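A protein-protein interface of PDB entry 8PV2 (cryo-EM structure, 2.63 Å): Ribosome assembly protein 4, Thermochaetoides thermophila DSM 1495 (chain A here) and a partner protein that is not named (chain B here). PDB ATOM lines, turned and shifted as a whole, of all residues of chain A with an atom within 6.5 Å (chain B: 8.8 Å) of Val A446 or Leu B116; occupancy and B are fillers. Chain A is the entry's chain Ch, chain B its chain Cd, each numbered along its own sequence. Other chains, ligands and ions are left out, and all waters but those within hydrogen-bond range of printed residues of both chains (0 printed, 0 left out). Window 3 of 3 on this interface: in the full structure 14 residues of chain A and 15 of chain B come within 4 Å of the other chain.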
ATOM      1  N   ASN A 426      12.331 -10.596   4.705  1.00  0.00           N
ATOM      2  CA  ASN A 426      11.906 -11.675   5.594  1.00  0.00           C
ATOM      3  C   ASN A 426      12.637 -11.672   6.927  1.00  0.00           C
ATOM      4  O   ASN A 426      12.692 -12.706   7.598  1.00  0.00           O
ATOM      5  CB  ASN A 426      12.069 -13.057   4.946  1.00  0.00           C
ATOM      6  CG  ASN A 426      11.471 -13.132   3.565  1.00  0.00           C
ATOM      7  OD1 ASN A 426      10.495 -12.462   3.260  1.00  0.00           O
ATOM      8  ND2 ASN A 426      12.042 -13.979   2.726  1.00  0.00           N
ATOM      9  N   ARG A 443      16.119 -14.604  11.905  1.00  0.00           N
ATOM     10  CA  ARG A 443      15.745 -15.280  10.672  1.00  0.00           C
ATOM     11  C   ARG A 443      14.735 -16.376  10.985  1.00  0.00           C
ATOM     12  O   ARG A 443      14.821 -17.019  12.034  1.00  0.00           O
ATOM     13  CB  ARG A 443      16.985 -15.865   9.999  1.00  0.00           C
ATOM     14  CG  ARG A 443      16.793 -16.304   8.565  1.00  0.00           C
ATOM     15  CD  ARG A 443      18.075 -16.895   8.018  1.00  0.00           C
ATOM     16  NE  ARG A 443      17.964 -17.254   6.610  1.00  0.00           N
ATOM     17  CZ  ARG A 443      18.923 -17.850   5.915  1.00  0.00           C
ATOM     18  NH1 ARG A 443      20.078 -18.175   6.472  1.00  0.00           N
ATOM     19  NH2 ARG A 443      18.718 -18.127   4.632  1.00  0.00           N
ATOM     20  N   GLY A 444      13.801 -16.605  10.067  1.00  0.00           N
ATOM     21  CA  GLY A 444      12.753 -17.576  10.306  1.00  0.00           C
ATOM     22  C   GLY A 444      11.404 -17.254   9.697  1.00  0.00           C
ATOM     23  O   GLY A 444      10.620 -18.167   9.431  1.00  0.00           O
ATOM     24  N   HIS A 445      11.108 -15.980   9.464  1.00  0.00           N
ATOM     25  CA  HIS A 445       9.948 -15.641   8.652  1.00  0.00           C
ATOM     26  C   HIS A 445      10.252 -15.921   7.184  1.00  0.00           C
ATOM     27  O   HIS A 445      11.388 -15.789   6.728  1.00  0.00           O
ATOM     28  CB  HIS A 445       9.566 -14.173   8.833  1.00  0.00           C
ATOM     29  CG  HIS A 445       8.757 -13.899  10.062  1.00  0.00           C
ATOM     30  ND1 HIS A 445       7.507 -14.435  10.267  1.00  0.00           N
ATOM     31  CD2 HIS A 445       9.019 -13.133  11.146  1.00  0.00           C
ATOM     32  CE1 HIS A 445       7.034 -14.016  11.426  1.00  0.00           C
ATOM     33  NE2 HIS A 445       7.932 -13.223  11.979  1.00  0.00           N
ATOM     34  N   VAL A 446       9.223 -16.318   6.440  1.00  0.00           N
ATOM     35  CA  VAL A 446       9.373 -16.657   5.031  1.00  0.00           C
ATOM     36  C   VAL A 446       8.625 -15.706   4.115  1.00  0.00           C
ATOM     37  O   VAL A 446       8.520 -15.976   2.917  1.00  0.00           O
ATOM     38  CB  VAL A 446       8.946 -18.112   4.753  1.00  0.00           C
ATOM     39  CG1 VAL A 446       9.978 -19.076   5.294  1.00  0.00           C
ATOM     40  CG2 VAL A 446       7.597 -18.397   5.356  1.00  0.00           C
ATOM     41  N   ALA A 447       8.103 -14.607   4.639  1.00  0.00           N
ATOM     42  CA  ALA A 447       7.431 -13.572   3.867  1.00  0.00           C
ATOM     43  C   ALA A 447       7.777 -12.234   4.509  1.00  0.00           C
ATOM     44  O   ALA A 447       8.339 -12.235   5.610  1.00  0.00           O
ATOM     45  CB  ALA A 447       5.925 -13.827   3.824  1.00  0.00           C
ATOM     46  N   PRO A 448       7.543 -11.078   3.831  1.00  0.00           N
ATOM     47  CA  PRO A 448       7.854  -9.775   4.443  1.00  0.00           C
ATOM     48  C   PRO A 448       7.265  -9.540   5.825  1.00  0.00           C
ATOM     49  O   PRO A 448       6.077  -9.765   6.061  1.00  0.00           O
ATOM     50  CB  PRO A 448       7.266  -8.786   3.436  1.00  0.00           C
ATOM     51  CG  PRO A 448       7.433  -9.452   2.150  1.00  0.00           C
ATOM     52  CD  PRO A 448       7.307 -10.929   2.382  1.00  0.00           C
ATOM     53  N   VAL A 449       8.108  -9.087   6.745  1.00  0.00           N
ATOM     54  CA  VAL A 449       7.718  -8.839   8.125  1.00  0.00           C
ATOM     55  C   VAL A 449       7.141  -7.437   8.194  1.00  0.00           C
ATOM     56  O   VAL A 449       7.828  -6.460   7.877  1.00  0.00           O
ATOM     57  CB  VAL A 449       8.909  -9.004   9.080  1.00  0.00           C
ATOM     58  CG1 VAL A 449       8.445  -8.960  10.508  1.00  0.00           C
ATOM     59  CG2 VAL A 449       9.600 -10.313   8.813  1.00  0.00           C
ATOM     60  N   SER A 465       4.137 -11.127  10.423  1.00  0.00           N
ATOM     61  CA  SER A 465       4.570 -11.089   9.036  1.00  0.00           C
ATOM     62  C   SER A 465       3.444 -11.430   8.071  1.00  0.00           C
ATOM     63  O   SER A 465       2.304 -11.696   8.454  1.00  0.00           O
ATOM     64  CB  SER A 465       5.743 -12.039   8.803  1.00  0.00           C
ATOM     65  OG  SER A 465       6.031 -12.149   7.425  1.00  0.00           O
ATOM     66  N   ASP A 467       3.583 -14.062   6.173  1.00  0.00           N
ATOM     67  CA  ASP A 467       3.455 -15.514   6.110  1.00  0.00           C
ATOM     68  C   ASP A 467       2.434 -16.069   7.090  1.00  0.00           C
ATOM     69  O   ASP A 467       2.485 -17.267   7.389  1.00  0.00           O
ATOM     70  CB  ASP A 467       4.816 -16.186   6.331  1.00  0.00           C
ATOM     71  CG  ASP A 467       5.440 -15.867   7.682  1.00  0.00           C
ATOM     72  OD1 ASP A 467       4.855 -15.123   8.488  1.00  0.00           O
ATOM     73  OD2 ASP A 467       6.549 -16.371   7.936  1.00  0.00           O
ATOM     74  N   THR A 469       2.042 -15.618  10.305  1.00  0.00           N
ATOM     75  CA  THR A 469       2.488 -16.013  11.631  1.00  0.00           C
ATOM     76  C   THR A 469       3.043 -14.829  12.415  1.00  0.00           C
ATOM     77  O   THR A 469       3.493 -13.811  11.855  1.00  0.00           O
ATOM     78  CB  THR A 469       3.562 -17.119  11.586  1.00  0.00           C
ATOM     79  OG1 THR A 469       4.809 -16.569  11.147  1.00  0.00           O
ATOM     80  CG2 THR A 469       3.159 -18.263  10.676  1.00  0.00           C
ATOM     81  N   LYS A 471       5.993 -14.318  15.495  1.00  0.00           N
ATOM     82  CA  LYS A 471       7.133 -14.980  16.108  1.00  0.00           C
ATOM     83  C   LYS A 471       7.668 -14.130  17.244  1.00  0.00           C
ATOM     84  O   LYS A 471       7.966 -12.949  17.058  1.00  0.00           O
ATOM     85  CB  LYS A 471       8.242 -15.257  15.097  1.00  0.00           C
ATOM     86  CG  LYS A 471       7.875 -16.250  14.025  1.00  0.00           C
ATOM     87  CD  LYS A 471       9.101 -16.793  13.348  1.00  0.00           C
ATOM     88  CE  LYS A 471       8.730 -17.560  12.113  1.00  0.00           C
ATOM     89  NZ  LYS A 471       7.663 -18.537  12.398  1.00  0.00           N
ATOM     90  N   VAL B  82       7.429 -30.747   3.845  1.00  0.00           N
ATOM     91  CA  VAL B  82       7.354 -29.764   4.914  1.00  0.00           C
ATOM     92  C   VAL B  82       8.617 -29.868   5.751  1.00  0.00           C
ATOM     93  O   VAL B  82       9.281 -30.908   5.781  1.00  0.00           O
ATOM     94  CB  VAL B  82       6.101 -29.953   5.793  1.00  0.00           C
ATOM     95  CG1 VAL B  82       4.853 -29.574   5.027  1.00  0.00           C
ATOM     96  CG2 VAL B  82       6.010 -31.383   6.274  1.00  0.00           C
ATOM     97  N   ILE B  83       8.957 -28.776   6.426  1.00  0.00           N
ATOM     98  CA  ILE B  83      10.145 -28.719   7.264  1.00  0.00           C
ATOM     99  C   ILE B  83       9.856 -27.794   8.437  1.00  0.00           C
ATOM    100  O   ILE B  83       9.086 -26.835   8.313  1.00  0.00           O
ATOM    101  CB  ILE B  83      11.385 -28.277   6.447  1.00  0.00           C
ATOM    102  CG1 ILE B  83      12.679 -28.495   7.234  1.00  0.00           C
ATOM    103  CG2 ILE B  83      11.259 -26.840   5.959  1.00  0.00           C
ATOM    104  CD1 ILE B  83      13.916 -28.440   6.388  1.00  0.00           C
ATOM    105  N   SER B  84      10.435 -28.107   9.591  1.00  0.00           N
ATOM    106  CA  SER B  84      10.207 -27.320  10.789  1.00  0.00           C
ATOM    107  C   SER B  84      11.318 -26.297  10.996  1.00  0.00           C
ATOM    108  O   SER B  84      12.384 -26.363  10.374  1.00  0.00           O
ATOM    109  CB  SER B  84      10.100 -28.231  12.009  1.00  0.00           C
ATOM    110  OG  SER B  84      11.355 -28.792  12.335  1.00  0.00           O
ATOM    111  N   GLN B  85      11.049 -25.340  11.887  1.00  0.00           N
ATOM    112  CA  GLN B  85      12.001 -24.264  12.137  1.00  0.00           C
ATOM    113  C   GLN B  85      13.251 -24.763  12.847  1.00  0.00           C
ATOM    114  O   GLN B  85      14.348 -24.255  12.593  1.00  0.00           O
ATOM    115  CB  GLN B  85      11.336 -23.157  12.951  1.00  0.00           C
ATOM    116  CG  GLN B  85      10.174 -22.481  12.253  1.00  0.00           C
ATOM    117  CD  GLN B  85      10.613 -21.413  11.277  1.00  0.00           C
ATOM    118  OE1 GLN B  85      11.799 -21.122  11.147  1.00  0.00           O
ATOM    119  NE2 GLN B  85       9.654 -20.817  10.589  1.00  0.00           N
ATOM    120  N   THR B  87      14.576 -27.784  12.448  1.00  0.00           N
ATOM    121  CA  THR B  87      15.344 -28.460  11.410  1.00  0.00           C
ATOM    122  C   THR B  87      16.030 -27.455  10.495  1.00  0.00           C
ATOM    123  O   THR B  87      17.198 -27.638  10.126  1.00  0.00           O
ATOM    124  CB  THR B  87      14.423 -29.382  10.616  1.00  0.00           C
ATOM    125  OG1 THR B  87      13.730 -30.247  11.522  1.00  0.00           O
ATOM    126  CG2 THR B  87      15.217 -30.230   9.662  1.00  0.00           C
ATOM    127  N   LEU B  88      15.327 -26.372  10.145  1.00  0.00           N
ATOM    128  CA  LEU B  88      15.939 -25.316   9.345  1.00  0.00           C
ATOM    129  C   LEU B  88      17.112 -24.671  10.067  1.00  0.00           C
ATOM    130  O   LEU B  88      18.147 -24.401   9.453  1.00  0.00           O
ATOM    131  CB  LEU B  88      14.906 -24.256   8.979  1.00  0.00           C
ATOM    132  CG  LEU B  88      14.065 -24.539   7.741  1.00  0.00           C
ATOM    133  CD1 LEU B  88      12.935 -23.538   7.636  1.00  0.00           C
ATOM    134  CD2 LEU B  88      14.936 -24.496   6.504  1.00  0.00           C
ATOM    135  N   GLN B  89      16.977 -24.421  11.371  1.00  0.00           N
ATOM    136  CA  GLN B  89      18.055 -23.774  12.111  1.00  0.00           C
ATOM    137  C   GLN B  89      19.269 -24.690  12.239  1.00  0.00           C
ATOM    138  O   GLN B  89      20.417 -24.231  12.146  1.00  0.00           O
ATOM    139  CB  GLN B  89      17.552 -23.331  13.484  1.00  0.00           C
ATOM    140  CG  GLN B  89      18.590 -22.610  14.324  1.00  0.00           C
ATOM    141  CD  GLN B  89      19.085 -21.328  13.676  1.00  0.00           C
ATOM    142  OE1 GLN B  89      18.340 -20.635  12.984  1.00  0.00           O
ATOM    143  NE2 GLN B  89      20.357 -21.014  13.890  1.00  0.00           N
ATOM    144  N   SER B  90      19.034 -25.991  12.435  1.00  0.00           N
ATOM    145  CA  SER B  90      20.135 -26.952  12.455  1.00  0.00           C
ATOM    146  C   SER B  90      20.846 -27.001  11.108  1.00  0.00           C
ATOM    147  O   SER B  90      22.081 -27.069  11.044  1.00  0.00           O
ATOM    148  CB  SER B  90      19.616 -28.335  12.839  1.00  0.00           C
ATOM    149  OG  SER B  90      19.002 -28.313  14.114  1.00  0.00           O
ATOM    150  N   PHE B  91      20.079 -26.952  10.017  1.00  0.00           N
ATOM    151  CA  PHE B  91      20.689 -26.942   8.693  1.00  0.00           C
ATOM    152  C   PHE B  91      21.467 -25.657   8.443  1.00  0.00           C
ATOM    153  O   PHE B  91      22.500 -25.675   7.769  1.00  0.00           O
ATOM    154  CB  PHE B  91      19.619 -27.139   7.625  1.00  0.00           C
ATOM    155  CG  PHE B  91      19.228 -28.568   7.426  1.00  0.00           C
ATOM    156  CD1 PHE B  91      20.176 -29.572   7.497  1.00  0.00           C
ATOM    157  CD2 PHE B  91      17.915 -28.910   7.174  1.00  0.00           C
ATOM    158  CE1 PHE B  91      19.820 -30.889   7.320  1.00  0.00           C
ATOM    159  CE2 PHE B  91      17.557 -30.227   6.994  1.00  0.00           C
ATOM    160  CZ  PHE B  91      18.509 -31.217   7.067  1.00  0.00           C
ATOM    161  N   ARG B  92      20.986 -24.529   8.971  1.00  0.00           N
ATOM    162  CA  ARG B  92      21.717 -23.271   8.825  1.00  0.00           C
ATOM    163  C   ARG B  92      23.035 -23.308   9.585  1.00  0.00           C
ATOM    164  O   ARG B  92      24.058 -22.806   9.098  1.00  0.00           O
ATOM    165  CB  ARG B  92      20.865 -22.101   9.305  1.00  0.00           C
ATOM    166  CG  ARG B  92      19.667 -21.808   8.438  1.00  0.00           C
ATOM    167  CD  ARG B  92      19.058 -20.470   8.771  1.00  0.00           C
ATOM    168  NE  ARG B  92      17.738 -20.321   8.176  1.00  0.00           N
ATOM    169  CZ  ARG B  92      16.602 -20.365   8.857  1.00  0.00           C
ATOM    170  NH1 ARG B  92      16.590 -20.495  10.171  1.00  0.00           N
ATOM    171  NH2 ARG B  92      15.451 -20.263   8.202  1.00  0.00           N
ATOM    172  N   GLU B  93      23.029 -23.895  10.784  1.00  0.00           N
ATOM    173  CA  GLU B  93      24.270 -24.049  11.537  1.00  0.00           C
ATOM    174  C   GLU B  93      25.248 -24.968  10.816  1.00  0.00           C
ATOM    175  O   GLU B  93      26.455 -24.698  10.780  1.00  0.00           O
ATOM    176  CB  GLU B  93      23.972 -24.574  12.937  1.00  0.00           C
ATOM    177  CG  GLU B  93      23.212 -23.593  13.799  1.00  0.00           C
ATOM    178  CD  GLU B  93      22.927 -24.138  15.177  1.00  0.00           C
ATOM    179  OE1 GLU B  93      23.254 -25.317  15.427  1.00  0.00           O
ATOM    180  OE2 GLU B  93      22.377 -23.390  16.011  1.00  0.00           O
ATOM    181  N   MET B  95      25.343 -25.358   7.574  1.00  0.00           N
ATOM    182  CA  MET B  95      25.784 -24.577   6.422  1.00  0.00           C
ATOM    183  C   MET B  95      26.901 -23.615   6.805  1.00  0.00           C
ATOM    184  O   MET B  95      27.855 -23.416   6.045  1.00  0.00           O
ATOM    185  CB  MET B  95      24.595 -23.812   5.844  1.00  0.00           C
ATOM    186  CG  MET B  95      24.725 -23.357   4.403  1.00  0.00           C
ATOM    187  SD  MET B  95      24.867 -24.680   3.198  1.00  0.00           S
ATOM    188  CE  MET B  95      26.247 -24.079   2.239  1.00  0.00           C
ATOM    189  N   LEU B 112      16.799 -30.443  -0.279  1.00  0.00           N
ATOM    190  CA  LEU B 112      16.571 -29.503   0.804  1.00  0.00           C
ATOM    191  C   LEU B 112      16.160 -28.162   0.223  1.00  0.00           C
ATOM    192  O   LEU B 112      16.516 -27.837  -0.913  1.00  0.00           O
ATOM    193  CB  LEU B 112      17.834 -29.338   1.658  1.00  0.00           C
ATOM    194  CG  LEU B 112      18.168 -30.491   2.591  1.00  0.00           C
ATOM    195  CD1 LEU B 112      19.410 -30.159   3.388  1.00  0.00           C
ATOM    196  CD2 LEU B 112      16.994 -30.778   3.500  1.00  0.00           C
ATOM    197  N   PRO B 113      15.404 -27.360   0.978  1.00  0.00           N
ATOM    198  CA  PRO B 113      15.090 -25.989   0.529  1.00  0.00           C
ATOM    199  C   PRO B 113      16.262 -25.042   0.768  1.00  0.00           C
ATOM    200  O   PRO B 113      16.353 -24.336   1.768  1.00  0.00           O
ATOM    201  CB  PRO B 113      13.870 -25.632   1.378  1.00  0.00           C
ATOM    202  CG  PRO B 113      14.032 -26.421   2.611  1.00  0.00           C
ATOM    203  CD  PRO B 113      14.712 -27.697   2.234  1.00  0.00           C
ATOM    204  N   MET B 114      17.193 -25.030  -0.190  1.00  0.00           N
ATOM    205  CA  MET B 114      18.457 -24.320  -0.007  1.00  0.00           C
ATOM    206  C   MET B 114      18.278 -22.813   0.082  1.00  0.00           C
ATOM    207  O   MET B 114      19.118 -22.133   0.677  1.00  0.00           O
ATOM    208  CB  MET B 114      19.424 -24.667  -1.137  1.00  0.00           C
ATOM    209  CG  MET B 114      19.851 -26.124  -1.189  1.00  0.00           C
ATOM    210  SD  MET B 114      20.144 -26.892   0.419  1.00  0.00           S
ATOM    211  CE  MET B 114      21.530 -25.942   1.049  1.00  0.00           C
ATOM    212  N   SER B 115      17.195 -22.272  -0.479  1.00  0.00           N
ATOM    213  CA  SER B 115      16.958 -20.836  -0.390  1.00  0.00           C
ATOM    214  C   SER B 115      16.666 -20.386   1.034  1.00  0.00           C
ATOM    215  O   SER B 115      16.883 -19.214   1.357  1.00  0.00           O
ATOM    216  CB  SER B 115      15.809 -20.429  -1.310  1.00  0.00           C
ATOM    217  OG  SER B 115      14.578 -20.964  -0.866  1.00  0.00           O
ATOM    218  N   LEU B 116      16.185 -21.283   1.890  1.00  0.00           N
ATOM    219  CA  LEU B 116      15.946 -20.979   3.292  1.00  0.00           C
ATOM    220  C   LEU B 116      17.106 -21.370   4.191  1.00  0.00           C
ATOM    221  O   LEU B 116      17.026 -21.161   5.404  1.00  0.00           O
ATOM    222  CB  LEU B 116      14.678 -21.682   3.774  1.00  0.00           C
ATOM    223  CG  LEU B 116      13.394 -21.445   2.989  1.00  0.00           C
ATOM    224  CD1 LEU B 116      12.341 -22.437   3.422  1.00  0.00           C
ATOM    225  CD2 LEU B 116      12.912 -20.028   3.188  1.00  0.00           C
ATOM    226  N   ILE B 117      18.174 -21.939   3.634  1.00  0.00           N
ATOM    227  CA  ILE B 117      19.271 -22.485   4.419  1.00  0.00           C
ATOM    228  C   ILE B 117      20.579 -21.754   4.157  1.00  0.00           C
ATOM    229  O   ILE B 117      21.327 -21.460   5.097  1.00  0.00           O
ATOM    230  CB  ILE B 117      19.429 -23.999   4.162  1.00  0.00           C
ATOM    231  CG1 ILE B 117      18.121 -24.718   4.481  1.00  0.00           C
ATOM    232  CG2 ILE B 117      20.534 -24.581   5.013  1.00  0.00           C
ATOM    233  CD1 ILE B 117      18.102 -26.163   4.076  1.00  0.00           C
ATOM    234  N   ARG B 118      20.877 -21.439   2.898  1.00  0.00           N
ATOM    235  CA  ARG B 118      22.102 -20.709   2.605  1.00  0.00           C
ATOM    236  C   ARG B 118      21.982 -19.267   3.081  1.00  0.00           C
ATOM    237  O   ARG B 118      20.882 -18.725   3.225  1.00  0.00           O
ATOM    238  CB  ARG B 118      22.414 -20.734   1.111  1.00  0.00           C
ATOM    239  CG  ARG B 118      21.426 -19.967   0.260  1.00  0.00           C
ATOM    240  CD  ARG B 118      21.840 -19.948  -1.196  1.00  0.00           C
ATOM    241  NE  ARG B 118      21.839 -21.274  -1.798  1.00  0.00           N
ATOM    242  CZ  ARG B 118      21.106 -21.615  -2.850  1.00  0.00           C
ATOM    243  NH1 ARG B 118      20.276 -20.758  -3.420  1.00  0.00           N
ATOM    244  NH2 ARG B 118      21.210 -22.846  -3.341  1.00  0.00           N
ATOM    245  N   ASP B 119      23.128 -18.650   3.344  1.00  0.00           N
ATOM    246  CA  ASP B 119      23.142 -17.273   3.809  1.00  0.00           C
ATOM    247  C   ASP B 119      22.745 -16.304   2.696  1.00  0.00           C
ATOM    248  O   ASP B 119      22.811 -16.616   1.504  1.00  0.00           O
ATOM    249  CB  ASP B 119      24.499 -16.955   4.466  1.00  0.00           C
ATOM    250  CG  ASP B 119      25.668 -16.692   3.478  1.00  0.00           C
ATOM    251  OD1 ASP B 119      25.541 -16.608   2.235  1.00  0.00           O
ATOM    252  OD2 ASP B 119      26.792 -16.559   4.002  1.00  0.00           O
ATOM    253  N   GLY B 120      22.312 -15.119   3.103  1.00  0.00           N
ATOM    254  CA  GLY B 120      21.913 -14.101   2.161  1.00  0.00           C
ATOM    255  C   GLY B 120      23.103 -13.474   1.475  1.00  0.00           C
ATOM    256  O   GLY B 120      24.266 -13.648   1.874  1.00  0.00           O
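Val A446 touches just one residue of chain B: Leu B116. No residue of chain B comes within 4 Å of Ala A447. Val A449 touches none of the printed residues of chain B. Of the printed residues of chain B, Lys A471 touches Gln B85 (3.5 Å). Printed residues of chain A within 4 Å of Gln B85: Gly A444 (3.0 Å) and Lys A471 (3.5 Å). Printed residues of chain A within 4 Å of Arg B92: Arg A443. Glu B93 touches none of the printed residues of chain A. Of the printed residues of chain A, Ser B115 touches Arg A443. Of chain A, only Arg A443 (3.6 Å) and Val A446 (3.7 Å) come within 4 Å of Leu B116. Printed residues of chain A within 4 Å of Ile B117: Arg A443. The nearest residue of chain B that does not touch Val A446 is Gln B85 (5.6 Å). The nearest printed residue of chain A that does not touch Arg B92 is Gly A444 (4.4 Å).
Among the printed residues, merely in contact across the chains: Lys A471 with Gln B85, Arg A443 with Leu B116, Val A446 with Leu B116, Arg A443 with Ile B117 and Arg A443 with Ser B115.
O of Arg B118 lies within hydrogen-bond range of NH2 of Arg A443. The guanidinium group (NE) of Arg A443 lies close to the guanidinium group (NE) of Arg B92, 3.5 Å away. The backbone carbonyl oxygen (O) of Gly A444 sits at hydrogen-bond distance from the side-chain amide nitrogen (NE2) of Gln B85, at 3.0 Å.
The backbone NH of Val A446 is in hydrogen-bond range of the side-chain carboxylate of Asp A467, 3.1 Å away. OE1 of Gln B89 sits at hydrogen-bond distance from NH1 of Arg B92, at 3.3 Å. The guanidinium group of Arg B92 lies within hydrogen-bond range of the backbone carbonyl oxygen of Leu B116 (3.0 Å).
Of the 12 printed residues of chain A, 4 touch a printed residue of chain B. Hydrophobic or aromatic side chains of chain A that line the printed part of chain B: Val A446. Of the 21 printed residues of chain B, 6 touch a printed residue of chain A. Among the printed residues, 8 pairs touch across the chains.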
